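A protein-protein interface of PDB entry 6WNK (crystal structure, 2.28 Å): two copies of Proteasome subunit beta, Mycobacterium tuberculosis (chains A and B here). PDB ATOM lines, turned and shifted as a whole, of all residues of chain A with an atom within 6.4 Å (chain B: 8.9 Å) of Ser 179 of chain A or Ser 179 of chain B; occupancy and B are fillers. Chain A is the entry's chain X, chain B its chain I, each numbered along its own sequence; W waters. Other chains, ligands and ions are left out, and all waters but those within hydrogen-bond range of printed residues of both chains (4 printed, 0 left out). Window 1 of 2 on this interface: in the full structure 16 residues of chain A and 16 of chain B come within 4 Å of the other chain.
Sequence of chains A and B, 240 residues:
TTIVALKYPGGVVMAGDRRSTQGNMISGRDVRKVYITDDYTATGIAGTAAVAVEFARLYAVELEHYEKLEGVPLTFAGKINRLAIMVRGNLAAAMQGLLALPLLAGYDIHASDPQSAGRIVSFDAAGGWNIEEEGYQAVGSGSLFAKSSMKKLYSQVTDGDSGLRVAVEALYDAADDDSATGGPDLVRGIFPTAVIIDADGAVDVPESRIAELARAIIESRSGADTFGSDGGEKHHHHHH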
ATOM      1  N   ARG A  19      17.732   1.916  -8.918  1.00  0.00           N
ATOM      2  CA  ARG A  19      18.575   2.017  -7.734  1.00  0.00           C
ATOM      3  C   ARG A  19      18.344   3.331  -6.997  1.00  0.00           C
ATOM      4  O   ARG A  19      18.162   4.383  -7.616  1.00  0.00           O
ATOM      5  CB  ARG A  19      20.052   1.890  -8.116  1.00  0.00           C
ATOM      6  CG  ARG A  19      21.030   2.187  -6.979  1.00  0.00           C
ATOM      7  CD  ARG A  19      22.426   1.668  -7.292  1.00  0.00           C
ATOM      8  NE  ARG A  19      22.424   0.214  -7.430  1.00  0.00           N
ATOM      9  CZ  ARG A  19      23.510  -0.518  -7.654  1.00  0.00           C
ATOM     10  NH1 ARG A  19      24.696   0.066  -7.770  1.00  0.00           N
ATOM     11  NH2 ARG A  19      23.407  -1.836  -7.761  1.00  0.00           N
ATOM     12  N   THR A  21      20.376   5.284  -3.579  1.00  0.00           N
ATOM     13  CA  THR A  21      21.528   5.193  -2.699  1.00  0.00           C
ATOM     14  C   THR A  21      21.437   6.260  -1.619  1.00  0.00           C
ATOM     15  O   THR A  21      20.729   7.264  -1.748  1.00  0.00           O
ATOM     16  CB  THR A  21      22.861   5.344  -3.459  1.00  0.00           C
ATOM     17  OG1 THR A  21      22.877   6.589  -4.168  1.00  0.00           O
ATOM     18  CG2 THR A  21      23.065   4.198  -4.442  1.00  0.00           C
ATOM     19  N   GLY A  23      24.575   7.797   0.030  1.00  0.00           N
ATOM     20  CA  GLY A  23      26.024   7.748   0.080  1.00  0.00           C
ATOM     21  C   GLY A  23      26.524   6.593  -0.771  1.00  0.00           C
ATOM     22  O   GLY A  23      26.067   6.370  -1.899  1.00  0.00           O
ATOM     23  N   ASN A  24      27.488   5.849  -0.234  1.00  0.00           N
ATOM     24  CA  ASN A  24      27.945   4.613  -0.859  1.00  0.00           C
ATOM     25  C   ASN A  24      26.976   3.458  -0.641  1.00  0.00           C
ATOM     26  O   ASN A  24      27.061   2.447  -1.350  1.00  0.00           O
ATOM     27  CB  ASN A  24      29.328   4.239  -0.316  1.00  0.00           C
ATOM     28  CG  ASN A  24      29.469   4.540   1.174  1.00  0.00           C
ATOM     29  OD1 ASN A  24      28.763   5.394   1.721  1.00  0.00           O
ATOM     30  ND2 ASN A  24      30.390   3.842   1.836  1.00  0.00           N
ATOM     31  N   MET A  25      26.059   3.588   0.313  1.00  0.00           N
ATOM     32  CA  MET A  25      25.168   2.494   0.666  1.00  0.00           C
ATOM     33  C   MET A  25      23.997   2.406  -0.304  1.00  0.00           C
ATOM     34  O   MET A  25      23.393   3.416  -0.669  1.00  0.00           O
ATOM     35  CB  MET A  25      24.655   2.672   2.092  1.00  0.00           C
ATOM     36  CG  MET A  25      25.755   2.552   3.133  1.00  0.00           C
ATOM     37  SD  MET A  25      25.131   2.739   4.806  1.00  0.00           S
ATOM     38  CE  MET A  25      23.724   1.633   4.751  1.00  0.00           C
ATOM     39  N   ILE A  26      23.688   1.184  -0.725  1.00  0.00           N
ATOM     40  CA  ILE A  26      22.511   0.935  -1.547  1.00  0.00           C
ATOM     41  C   ILE A  26      21.293   0.931  -0.635  1.00  0.00           C
ATOM     42  O   ILE A  26      21.229   0.165   0.333  1.00  0.00           O
ATOM     43  CB  ILE A  26      22.646  -0.386  -2.316  1.00  0.00           C
ATOM     44  CG1 ILE A  26      23.782  -0.278  -3.334  1.00  0.00           C
ATOM     45  CG2 ILE A  26      21.339  -0.734  -3.017  1.00  0.00           C
ATOM     46  CD1 ILE A  26      24.339  -1.606  -3.778  1.00  0.00           C
ATOM     47  N   ALA A 174      25.404   2.597 -18.738  1.00  0.00           N
ATOM     48  CA  ALA A 174      25.444   3.569 -17.652  1.00  0.00           C
ATOM     49  C   ALA A 174      25.749   2.891 -16.324  1.00  0.00           C
ATOM     50  O   ALA A 174      26.623   3.338 -15.572  1.00  0.00           O
ATOM     51  CB  ALA A 174      24.118   4.331 -17.579  1.00  0.00           C
ATOM     52  N   ALA A 175      25.044   1.795 -16.024  1.00  0.00           N
ATOM     53  CA  ALA A 175      25.308   1.070 -14.784  1.00  0.00           C
ATOM     54  C   ALA A 175      26.686   0.424 -14.801  1.00  0.00           C
ATOM     55  O   ALA A 175      27.300   0.243 -13.743  1.00  0.00           O
ATOM     56  CB  ALA A 175      24.229   0.015 -14.548  1.00  0.00           C
ATOM     57  N   ASP A 176      27.177   0.064 -15.986  1.00  0.00           N
ATOM     58  CA  ASP A 176      28.520  -0.488 -16.102  1.00  0.00           C
ATOM     59  C   ASP A 176      29.575   0.493 -15.600  1.00  0.00           C
ATOM     60  O   ASP A 176      30.589   0.078 -15.032  1.00  0.00           O
ATOM     61  CB  ASP A 176      28.785  -0.859 -17.562  1.00  0.00           C
ATOM     62  CG  ASP A 176      29.809  -1.962 -17.716  1.00  0.00           C
ATOM     63  OD1 ASP A 176      30.102  -2.655 -16.721  1.00  0.00           O
ATOM     64  OD2 ASP A 176      30.322  -2.135 -18.840  1.00  0.00           O
ATOM     65  N   ASP A 177      29.351   1.796 -15.784  1.00  0.00           N
ATOM     66  CA  ASP A 177      30.351   2.804 -15.459  1.00  0.00           C
ATOM     67  C   ASP A 177      29.980   3.696 -14.282  1.00  0.00           C
ATOM     68  O   ASP A 177      30.861   4.380 -13.751  1.00  0.00           O
ATOM     69  CB  ASP A 177      30.632   3.686 -16.685  1.00  0.00           C
ATOM     70  CG  ASP A 177      31.372   2.937 -17.787  1.00  0.00           C
ATOM     71  OD1 ASP A 177      32.308   2.180 -17.464  1.00  0.00           O
ATOM     72  OD2 ASP A 177      31.010   3.097 -18.975  1.00  0.00           O
ATOM     73  N   ASP A 178      28.715   3.710 -13.859  1.00  0.00           N
ATOM     74  CA  ASP A 178      28.240   4.583 -12.789  1.00  0.00           C
ATOM     75  C   ASP A 178      27.634   3.727 -11.682  1.00  0.00           C
ATOM     76  O   ASP A 178      26.567   3.130 -11.866  1.00  0.00           O
ATOM     77  CB  ASP A 178      27.215   5.583 -13.319  1.00  0.00           C
ATOM     78  CG  ASP A 178      26.514   6.345 -12.207  1.00  0.00           C
ATOM     79  OD1 ASP A 178      27.138   6.576 -11.146  1.00  0.00           O
ATOM     80  OD2 ASP A 178      25.330   6.707 -12.388  1.00  0.00           O
ATOM     81  N   SER A 179      28.295   3.700 -10.523  1.00  0.00           N
ATOM     82  CA  SER A 179      27.827   2.874  -9.415  1.00  0.00           C
ATOM     83  C   SER A 179      26.502   3.356  -8.836  1.00  0.00           C
ATOM     84  O   SER A 179      25.860   2.602  -8.095  1.00  0.00           O
ATOM     85  CB  SER A 179      28.887   2.821  -8.311  1.00  0.00           C
ATOM     86  OG  SER A 179      29.061   4.090  -7.711  1.00  0.00           O
ATOM     87  N   ALA A 180      26.077   4.580  -9.147  1.00  0.00           N
ATOM     88  CA  ALA A 180      24.799   5.106  -8.686  1.00  0.00           C
ATOM     89  C   ALA A 180      23.649   4.779  -9.631  1.00  0.00           C
ATOM     90  O   ALA A 180      22.524   5.234  -9.400  1.00  0.00           O
ATOM     91  CB  ALA A 180      24.887   6.626  -8.493  1.00  0.00           C
ATOM     92  N   THR A 181      23.909   4.024 -10.691  1.00  0.00           N
ATOM     93  CA  THR A 181      22.882   3.516 -11.587  1.00  0.00           C
ATOM     94  C   THR A 181      22.861   1.997 -11.476  1.00  0.00           C
ATOM     95  O   THR A 181      23.909   1.348 -11.566  1.00  0.00           O
ATOM     96  CB  THR A 181      23.153   3.948 -13.031  1.00  0.00           C
ATOM     97  OG1 THR A 181      23.192   5.381 -13.113  1.00  0.00           O
ATOM     98  CG2 THR A 181      22.080   3.416 -13.957  1.00  0.00           C
ATOM     99  N   GLY A 182      21.675   1.428 -11.269  1.00  0.00           N
ATOM    100  CA  GLY A 182      21.573  -0.007 -11.042  1.00  0.00           C
ATOM    101  C   GLY A 182      21.520  -0.793 -12.341  1.00  0.00           C
ATOM    102  O   GLY A 182      20.766  -0.453 -13.258  1.00  0.00           O
ATOM    103  N   THR B   1      35.619  -0.446  -1.007  1.00  0.00           N
ATOM    104  CA  THR B   1      36.434  -1.626  -0.734  1.00  0.00           C
ATOM    105  C   THR B   1      35.856  -2.464   0.399  1.00  0.00           C
ATOM    106  O   THR B   1      35.280  -1.935   1.347  1.00  0.00           O
ATOM    107  CB  THR B   1      37.888  -1.233  -0.362  1.00  0.00           C
ATOM    108  OG1 THR B   1      38.505  -0.569  -1.468  1.00  0.00           O
ATOM    109  CG2 THR B   1      38.723  -2.457   0.015  1.00  0.00           C
ATOM    110  N   THR B   2      36.002  -3.779   0.291  1.00  0.00           N
ATOM    111  CA  THR B   2      35.872  -4.645   1.452  1.00  0.00           C
ATOM    112  C   THR B   2      36.998  -5.664   1.414  1.00  0.00           C
ATOM    113  O   THR B   2      37.256  -6.270   0.369  1.00  0.00           O
ATOM    114  CB  THR B   2      34.514  -5.351   1.501  1.00  0.00           C
ATOM    115  OG1 THR B   2      33.464  -4.382   1.407  1.00  0.00           O
ATOM    116  CG2 THR B   2      34.371  -6.109   2.817  1.00  0.00           C
ATOM    117  N   ASP B  17      37.830  -7.440  -2.638  1.00  0.00           N
ATOM    118  CA  ASP B  17      37.118  -7.145  -3.875  1.00  0.00           C
ATOM    119  C   ASP B  17      38.052  -6.469  -4.882  1.00  0.00           C
ATOM    120  O   ASP B  17      39.232  -6.224  -4.612  1.00  0.00           O
ATOM    121  CB  ASP B  17      35.893  -6.280  -3.596  1.00  0.00           C
ATOM    122  CG  ASP B  17      36.242  -4.819  -3.390  1.00  0.00           C
ATOM    123  OD1 ASP B  17      37.042  -4.511  -2.479  1.00  0.00           O
ATOM    124  OD2 ASP B  17      35.716  -3.974  -4.149  1.00  0.00           O
ATOM    125  N   ARG B  19      37.236  -3.532  -6.950  1.00  0.00           N
ATOM    126  CA  ARG B  19      36.719  -2.266  -7.459  1.00  0.00           C
ATOM    127  C   ARG B  19      37.565  -1.071  -7.020  1.00  0.00           C
ATOM    128  O   ARG B  19      38.051  -1.016  -5.889  1.00  0.00           O
ATOM    129  CB  ARG B  19      35.271  -2.064  -7.001  1.00  0.00           C
ATOM    130  CG  ARG B  19      34.664  -0.720  -7.368  1.00  0.00           C
ATOM    131  CD  ARG B  19      33.140  -0.757  -7.289  1.00  0.00           C
ATOM    132  NE  ARG B  19      32.570  -1.522  -8.393  1.00  0.00           N
ATOM    133  CZ  ARG B  19      31.269  -1.713  -8.590  1.00  0.00           C
ATOM    134  NH1 ARG B  19      30.379  -1.202  -7.748  1.00  0.00           N
ATOM    135  NH2 ARG B  19      30.857  -2.421  -9.635  1.00  0.00           N
ATOM    136  N   SER B  20      37.737  -0.115  -7.933  1.00  0.00           N
ATOM    137  CA  SER B  20      38.158   1.235  -7.588  1.00  0.00           C
ATOM    138  C   SER B  20      37.166   2.218  -8.194  1.00  0.00           C
ATOM    139  O   SER B  20      36.610   1.971  -9.268  1.00  0.00           O
ATOM    140  CB  SER B  20      39.587   1.553  -8.075  1.00  0.00           C
ATOM    141  OG  SER B  20      39.628   1.781  -9.472  1.00  0.00           O
ATOM    142  N   THR B  21      36.940   3.329  -7.493  1.00  0.00           N
ATOM    143  CA  THR B  21      35.991   4.348  -7.921  1.00  0.00           C
ATOM    144  C   THR B  21      36.624   5.733  -7.842  1.00  0.00           C
ATOM    145  O   THR B  21      37.639   5.941  -7.172  1.00  0.00           O
ATOM    146  CB  THR B  21      34.704   4.329  -7.068  1.00  0.00           C
ATOM    147  OG1 THR B  21      35.042   4.414  -5.678  1.00  0.00           O
ATOM    148  CG2 THR B  21      33.904   3.058  -7.315  1.00  0.00           C
ATOM    149  N   GLN B  22      36.010   6.678  -8.551  1.00  0.00           N
ATOM    150  CA  GLN B  22      36.258   8.112  -8.391  1.00  0.00           C
ATOM    151  C   GLN B  22      34.889   8.756  -8.213  1.00  0.00           C
ATOM    152  O   GLN B  22      34.205   9.047  -9.197  1.00  0.00           O
ATOM    153  CB  GLN B  22      36.983   8.713  -9.588  1.00  0.00           C
ATOM    154  CG  GLN B  22      38.435   8.322  -9.720  1.00  0.00           C
ATOM    155  CD  GLN B  22      39.183   9.225 -10.686  1.00  0.00           C
ATOM    156  OE1 GLN B  22      38.741  10.334 -10.983  1.00  0.00           O
ATOM    157  NE2 GLN B  22      40.319   8.750 -11.181  1.00  0.00           N
ATOM    158  N   GLY B  23      34.482   8.969  -6.968  1.00  0.00           N
ATOM    159  CA  GLY B  23      33.121   9.419  -6.732  1.00  0.00           C
ATOM    160  C   GLY B  23      32.145   8.311  -7.081  1.00  0.00           C
ATOM    161  O   GLY B  23      32.282   7.166  -6.629  1.00  0.00           O
ATOM    162  N   ASN B  24      31.146   8.644  -7.902  1.00  0.00           N
ATOM    163  CA  ASN B  24      30.197   7.642  -8.370  1.00  0.00           C
ATOM    164  C   ASN B  24      30.770   6.760  -9.467  1.00  0.00           C
ATOM    165  O   ASN B  24      30.264   5.652  -9.682  1.00  0.00           O
ATOM    166  CB  ASN B  24      28.922   8.316  -8.880  1.00  0.00           C
ATOM    167  CG  ASN B  24      28.001   8.748  -7.756  1.00  0.00           C
ATOM    168  OD1 ASN B  24      27.954   8.114  -6.699  1.00  0.00           O
ATOM    169  ND2 ASN B  24      27.260   9.830  -7.977  1.00  0.00           N
ATOM    170  N   MET B  25      31.816   7.218 -10.150  1.00  0.00           N
ATOM    171  CA  MET B  25      32.290   6.553 -11.352  1.00  0.00           C
ATOM    172  C   MET B  25      33.214   5.390 -11.022  1.00  0.00           C
ATOM    173  O   MET B  25      34.095   5.497 -10.165  1.00  0.00           O
ATOM    174  CB  MET B  25      33.008   7.554 -12.250  1.00  0.00           C
ATOM    175  CG  MET B  25      32.120   8.704 -12.697  1.00  0.00           C
ATOM    176  SD  MET B  25      32.993   9.782 -13.831  1.00  0.00           S
ATOM    177  CE  MET B  25      34.080   8.574 -14.586  1.00  0.00           C
ATOM    178  N   ILE B  26      33.000   4.273 -11.710  1.00  0.00           N
ATOM    179  CA  ILE B  26      33.865   3.106 -11.593  1.00  0.00           C
ATOM    180  C   ILE B  26      35.115   3.357 -12.425  1.00  0.00           C
ATOM    181  O   ILE B  26      35.030   3.610 -13.631  1.00  0.00           O
ATOM    182  CB  ILE B  26      33.141   1.834 -12.058  1.00  0.00           C
ATOM    183  CG1 ILE B  26      31.928   1.549 -11.170  1.00  0.00           C
ATOM    184  CG2 ILE B  26      34.092   0.654 -12.071  1.00  0.00           C
ATOM    185  CD1 ILE B  26      30.942   0.580 -11.781  1.00  0.00           C
ATOM    186  N   SER B  27      36.279   3.288 -11.784  1.00  0.00           N
ATOM    187  CA  SER B  27      37.546   3.543 -12.452  1.00  0.00           C
ATOM    188  C   SER B  27      38.437   2.315 -12.520  1.00  0.00           C
ATOM    189  O   SER B  27      39.516   2.388 -13.112  1.00  0.00           O
ATOM    190  CB  SER B  27      38.298   4.685 -11.755  1.00  0.00           C
ATOM    191  OG  SER B  27      38.726   4.300 -10.460  1.00  0.00           O
ATOM    192  N   GLY B  28      38.025   1.197 -11.925  1.00  0.00           N
ATOM    193  CA  GLY B  28      38.822  -0.014 -11.962  1.00  0.00           C
ATOM    194  C   GLY B  28      37.970  -1.222 -11.657  1.00  0.00           C
ATOM    195  O   GLY B  28      37.044  -1.159 -10.844  1.00  0.00           O
ATOM    196  N   ARG B  29      38.285  -2.336 -12.323  1.00  0.00           N
ATOM    197  CA  ARG B  29      37.525  -3.576 -12.180  1.00  0.00           C
ATOM    198  C   ARG B  29      38.369  -4.788 -11.830  1.00  0.00           C
ATOM    199  O   ARG B  29      37.802  -5.861 -11.595  1.00  0.00           O
ATOM    200  CB  ARG B  29      36.762  -3.894 -13.473  1.00  0.00           C
ATOM    201  CG  ARG B  29      35.815  -2.815 -13.912  1.00  0.00           C
ATOM    202  CD  ARG B  29      34.919  -3.310 -15.031  1.00  0.00           C
ATOM    203  NE  ARG B  29      33.852  -2.353 -15.293  1.00  0.00           N
ATOM    204  CZ  ARG B  29      33.959  -1.341 -16.144  1.00  0.00           C
ATOM    205  NH1 ARG B  29      35.082  -1.171 -16.827  1.00  0.00           N
ATOM    206  NH2 ARG B  29      32.944  -0.507 -16.322  1.00  0.00           N
ATOM    207  N   SER B 141      34.692   0.185   3.258  1.00  0.00           N
ATOM    208  CA  SER B 141      33.346   0.740   3.264  1.00  0.00           C
ATOM    209  C   SER B 141      32.254  -0.322   3.376  1.00  0.00           C
ATOM    210  O   SER B 141      31.133   0.005   3.774  1.00  0.00           O
ATOM    211  CB  SER B 141      33.130   1.559   1.991  1.00  0.00           C
ATOM    212  OG  SER B 141      33.459   0.789   0.851  1.00  0.00           O
ATOM    213  N   GLY B 142      32.536  -1.569   3.018  1.00  0.00           N
ATOM    214  CA  GLY B 142      31.535  -2.611   3.156  1.00  0.00           C
ATOM    215  C   GLY B 142      31.832  -3.543   4.312  1.00  0.00           C
ATOM    216  O   GLY B 142      31.266  -4.636   4.398  1.00  0.00           O
ATOM    217  N   PHE B 145      28.906  -4.623   6.689  1.00  0.00           N
ATOM    218  CA  PHE B 145      28.048  -5.626   6.064  1.00  0.00           C
ATOM    219  C   PHE B 145      28.728  -6.988   6.045  1.00  0.00           C
ATOM    220  O   PHE B 145      28.090  -8.015   6.315  1.00  0.00           O
ATOM    221  CB  PHE B 145      27.680  -5.210   4.640  1.00  0.00           C
ATOM    222  CG  PHE B 145      26.969  -3.892   4.549  1.00  0.00           C
ATOM    223  CD1 PHE B 145      25.689  -3.738   5.058  1.00  0.00           C
ATOM    224  CD2 PHE B 145      27.568  -2.816   3.918  1.00  0.00           C
ATOM    225  CE1 PHE B 145      25.028  -2.520   4.957  1.00  0.00           C
ATOM    226  CE2 PHE B 145      26.922  -1.594   3.818  1.00  0.00           C
ATOM    227  CZ  PHE B 145      25.650  -1.445   4.339  1.00  0.00           C
ATOM    228  N   ASP B 173      28.041 -10.306   0.142  1.00  0.00           N
ATOM    229  CA  ASP B 173      27.083  -9.512   0.903  1.00  0.00           C
ATOM    230  C   ASP B 173      27.514  -8.050   1.004  1.00  0.00           C
ATOM    231  O   ASP B 173      26.668  -7.146   1.001  1.00  0.00           O
ATOM    232  CB  ASP B 173      26.898 -10.115   2.296  1.00  0.00           C
ATOM    233  CG  ASP B 173      26.005 -11.344   2.285  1.00  0.00           C
ATOM    234  OD1 ASP B 173      24.977 -11.332   1.575  1.00  0.00           O
ATOM    235  OD2 ASP B 173      26.332 -12.319   2.989  1.00  0.00           O
ATOM    236  N   ALA B 174      28.821  -7.796   1.103  1.00  0.00           N
ATOM    237  CA  ALA B 174      29.286  -6.412   1.147  1.00  0.00           C
ATOM    238  C   ALA B 174      28.998  -5.702  -0.169  1.00  0.00           C
ATOM    239  O   ALA B 174      28.521  -4.561  -0.178  1.00  0.00           O
ATOM    240  CB  ALA B 174      30.781  -6.364   1.471  1.00  0.00           C
ATOM    241  N   ALA B 175      29.257  -6.375  -1.290  1.00  0.00           N
ATOM    242  CA  ALA B 175      28.956  -5.791  -2.589  1.00  0.00           C
ATOM    243  C   ALA B 175      27.462  -5.612  -2.781  1.00  0.00           C
ATOM    244  O   ALA B 175      27.032  -4.698  -3.493  1.00  0.00           O
ATOM    245  CB  ALA B 175      29.530  -6.670  -3.695  1.00  0.00           C
ATOM    246  N   ASP B 176      26.661  -6.472  -2.147  1.00  0.00           N
ATOM    247  CA  ASP B 176      25.212  -6.377  -2.249  1.00  0.00           C
ATOM    248  C   ASP B 176      24.695  -5.060  -1.679  1.00  0.00           C
ATOM    249  O   ASP B 176      23.693  -4.521  -2.165  1.00  0.00           O
ATOM    250  CB  ASP B 176      24.582  -7.563  -1.513  1.00  0.00           C
ATOM    251  CG  ASP B 176      23.265  -7.990  -2.111  1.00  0.00           C
ATOM    252  OD1 ASP B 176      22.953  -7.563  -3.243  1.00  0.00           O
ATOM    253  OD2 ASP B 176      22.541  -8.760  -1.448  1.00  0.00           O
ATOM    254  N   ASP B 177      25.371  -4.519  -0.665  1.00  0.00           N
ATOM    255  CA  ASP B 177      24.894  -3.344   0.050  1.00  0.00           C
ATOM    256  C   ASP B 177      25.795  -2.121  -0.091  1.00  0.00           C
ATOM    257  O   ASP B 177      25.354  -1.014   0.225  1.00  0.00           O
ATOM    258  CB  ASP B 177      24.716  -3.677   1.543  1.00  0.00           C
ATOM    259  CG  ASP B 177      23.453  -4.503   1.819  1.00  0.00           C
ATOM    260  OD1 ASP B 177      22.406  -4.210   1.203  1.00  0.00           O
ATOM    261  OD2 ASP B 177      23.503  -5.440   2.648  1.00  0.00           O
ATOM    262  N   ASP B 178      27.038  -2.283  -0.542  1.00  0.00           N
ATOM    263  CA  ASP B 178      27.997  -1.185  -0.634  1.00  0.00           C
ATOM    264  C   ASP B 178      28.401  -1.012  -2.092  1.00  0.00           C
ATOM    265  O   ASP B 178      29.116  -1.854  -2.646  1.00  0.00           O
ATOM    266  CB  ASP B 178      29.226  -1.448   0.236  1.00  0.00           C
ATOM    267  CG  ASP B 178      30.318  -0.411   0.028  1.00  0.00           C
ATOM    268  OD1 ASP B 178      29.991   0.740  -0.327  1.00  0.00           O
ATOM    269  OD2 ASP B 178      31.509  -0.747   0.205  1.00  0.00           O
ATOM    270  N   SER B 179      27.976   0.099  -2.695  1.00  0.00           N
ATOM    271  CA  SER B 179      28.294   0.359  -4.094  1.00  0.00           C
ATOM    272  C   SER B 179      29.786   0.592  -4.336  1.00  0.00           C
ATOM    273  O   SER B 179      30.219   0.550  -5.491  1.00  0.00           O
ATOM    274  CB  SER B 179      27.490   1.560  -4.593  1.00  0.00           C
ATOM    275  OG  SER B 179      27.884   2.747  -3.927  1.00  0.00           O
ATOM    276  N   ALA B 180      30.577   0.838  -3.290  1.00  0.00           N
ATOM    277  CA  ALA B 180      32.023   0.981  -3.427  1.00  0.00           C
ATOM    278  C   ALA B 180      32.764  -0.347  -3.327  1.00  0.00           C
ATOM    279  O   ALA B 180      33.999  -0.364  -3.376  1.00  0.00           O
ATOM    280  CB  ALA B 180      32.568   1.950  -2.372  1.00  0.00           C
ATOM    281  N   THR B 181      32.046  -1.452  -3.176  1.00  0.00           N
ATOM    282  CA  THR B 181      32.630  -2.784  -3.170  1.00  0.00           C
ATOM    283  C   THR B 181      32.111  -3.541  -4.383  1.00  0.00           C
ATOM    284  O   THR B 181      30.902  -3.541  -4.650  1.00  0.00           O
ATOM    285  CB  THR B 181      32.288  -3.523  -1.874  1.00  0.00           C
ATOM    286  OG1 THR B 181      32.884  -2.837  -0.762  1.00  0.00           O
ATOM    287  CG2 THR B 181      32.794  -4.956  -1.913  1.00  0.00           C
ATOM    288  N   GLY B 182      33.024  -4.171  -5.122  1.00  0.00           N
ATOM    289  CA  GLY B 182      32.676  -4.828  -6.369  1.00  0.00           C
ATOM    290  C   GLY B 182      32.212  -6.259  -6.169  1.00  0.00           C
ATOM    291  O   GLY B 182      32.877  -7.050  -5.498  1.00  0.00           O
ATOM    292  N   GLY B 183      31.072  -6.584  -6.756  1.00  0.00           N
ATOM    293  CA  GLY B 183      30.602  -7.948  -6.759  1.00  0.00           C
ATOM    294  C   GLY B 183      31.289  -8.771  -7.822  1.00  0.00           C
ATOM    295  O   GLY B 183      32.074  -8.272  -8.645  1.00  0.00           O
HETATM  296  O   HOH W   1      30.850   4.031  -5.211  1.00  0.00           O
HETATM  297  O   HOH W   2      33.809   5.075 -15.395  1.00  0.00           O
HETATM  298  O   HOH W   3      22.947  -0.483   2.056  1.00  0.00           O
HETATM  299  O   HOH W   4      26.890   5.111  -5.416  1.00  0.00           O
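OG of Ser 179 of chain B is in hydrogen-bond range of O of Asn 24 of chain A (2.7 Å).
N of Ile 26 of chain B is in hydrogen-bond range of O of Asp 177 of chain A (3.0 Å).
NH2 of Arg 29 of chain B is in salt-bridge range of OD1 of Asp 177 of chain A (3.0 Å).
OG of Ser 179 of chain A lies within hydrogen-bond range of O of Asn 24 of chain B, 2.8 Å away.
The side-chain carboxylate of Asp 176 of chain A is in salt-bridge range of the guanidinium group of Arg 29 of chain B, at 3.6 Å.
The backbone carbonyl oxygen of Asp 177 of chain B sits at hydrogen-bond distance from the backbone NH of Ile 26 of chain A, 2.9 Å away.
The backbone carbonyl oxygen (O) of Ser 179 of chain A sits at hydrogen-bond distance from the guanidinium group (NH1) of Arg 19 of chain A, 2.8 Å away.
OD1 of Asp 178 of chain A sits at hydrogen-bond distance from N of Ala 180 of chain A (3.0 Å).
Among the printed residues, pairs that only touch across the chains: Asp 176 of chain A with Ile 26 of chain B, Asp 178 of chain A with Asn 24 of chain B, Ile 26 of chain A with Asp 176 of chain B, Asp 177 of chain A with Met 25 of chain B, Met 25 of chain A with Asp 177 of chain B, Asn 24 of chain A with Asp 178 of chain B, Asn 24 of chain A with Ser 141 of chain B, Met 25 of chain A with Phe 145 of chain B, Ala 180 of chain A with Asn 24 of chain B and Ser 179 of chain A with Ser 179 of chain B.
Ser 179 of chain A touches just these residues of chain B: Asn 24 (2.8 Å) and Ser 179 (3.9 Å).
Of chain A, only Asn 24 and Ser 179 come within 4 Å of Ser 179 of chain B.
Of chain B, only Asn 24 comes within 4 Å of Asp 178 of chain A.
Of chain B, only Asn 24 comes within 4 Å of Ala 180 of chain A.
Of the printed residues of chain B, Asn 24 of chain A touches Ser 141 (3.6 Å), Asp 178 (3.5 Å) and Ser 179 (2.7 Å).
Ala 174 of chain A touches none of the printed residues of chain B.
Gly 23 of chain B touches none of the printed residues of chain A.
The nearest residue of chain B that does not touch Ser 179 of chain A is Ile 26 of chain B (4.3 Å).
The nearest residue of chain A that does not touch Ser 179 of chain B is Ile 26 of chain A (4.2 Å).
The nearest printed residue of chain A that does not touch Ile 26 of chain B is Ala 175 of chain A (4.2 Å).
Of the 15 printed residues of chain A, 8 touch a printed residue of chain B.
Hydrophobic or aromatic side chains of chain A that line the printed part of chain B: Met 25, Ile 26 and Ala 180.
Of the 28 printed residues of chain B, 10 touch a printed residue of chain A.
Hydrophobic or aromatic side chains of chain B within 4 Å of the printed part of chain A: Ile 26 and Phe 145.
Among the printed residues, 16 pairs touch across the chains.
Asn 24 of chain A touches Asp 178 of chain B, and with the chains exchanged Asp 178 of chain A touches Asn 24 of chain B.
Asn 24 of chain A touches Ser 179 of chain B, and with the chains exchanged Ser 179 of chain A touches Asn 24 of chain B.
15 positions are printed for both chains.
Water W4 lies within hydrogen-bond range of the side-chain hydroxyl (OG) of Ser 179 of chain B (3.0 Å), the side-chain hydroxyl (OG) of Ser 179 of chain A (3.3 Å) and the side-chain amide oxygen (OD1) of Asn 24 of chain B (3.4 Å).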
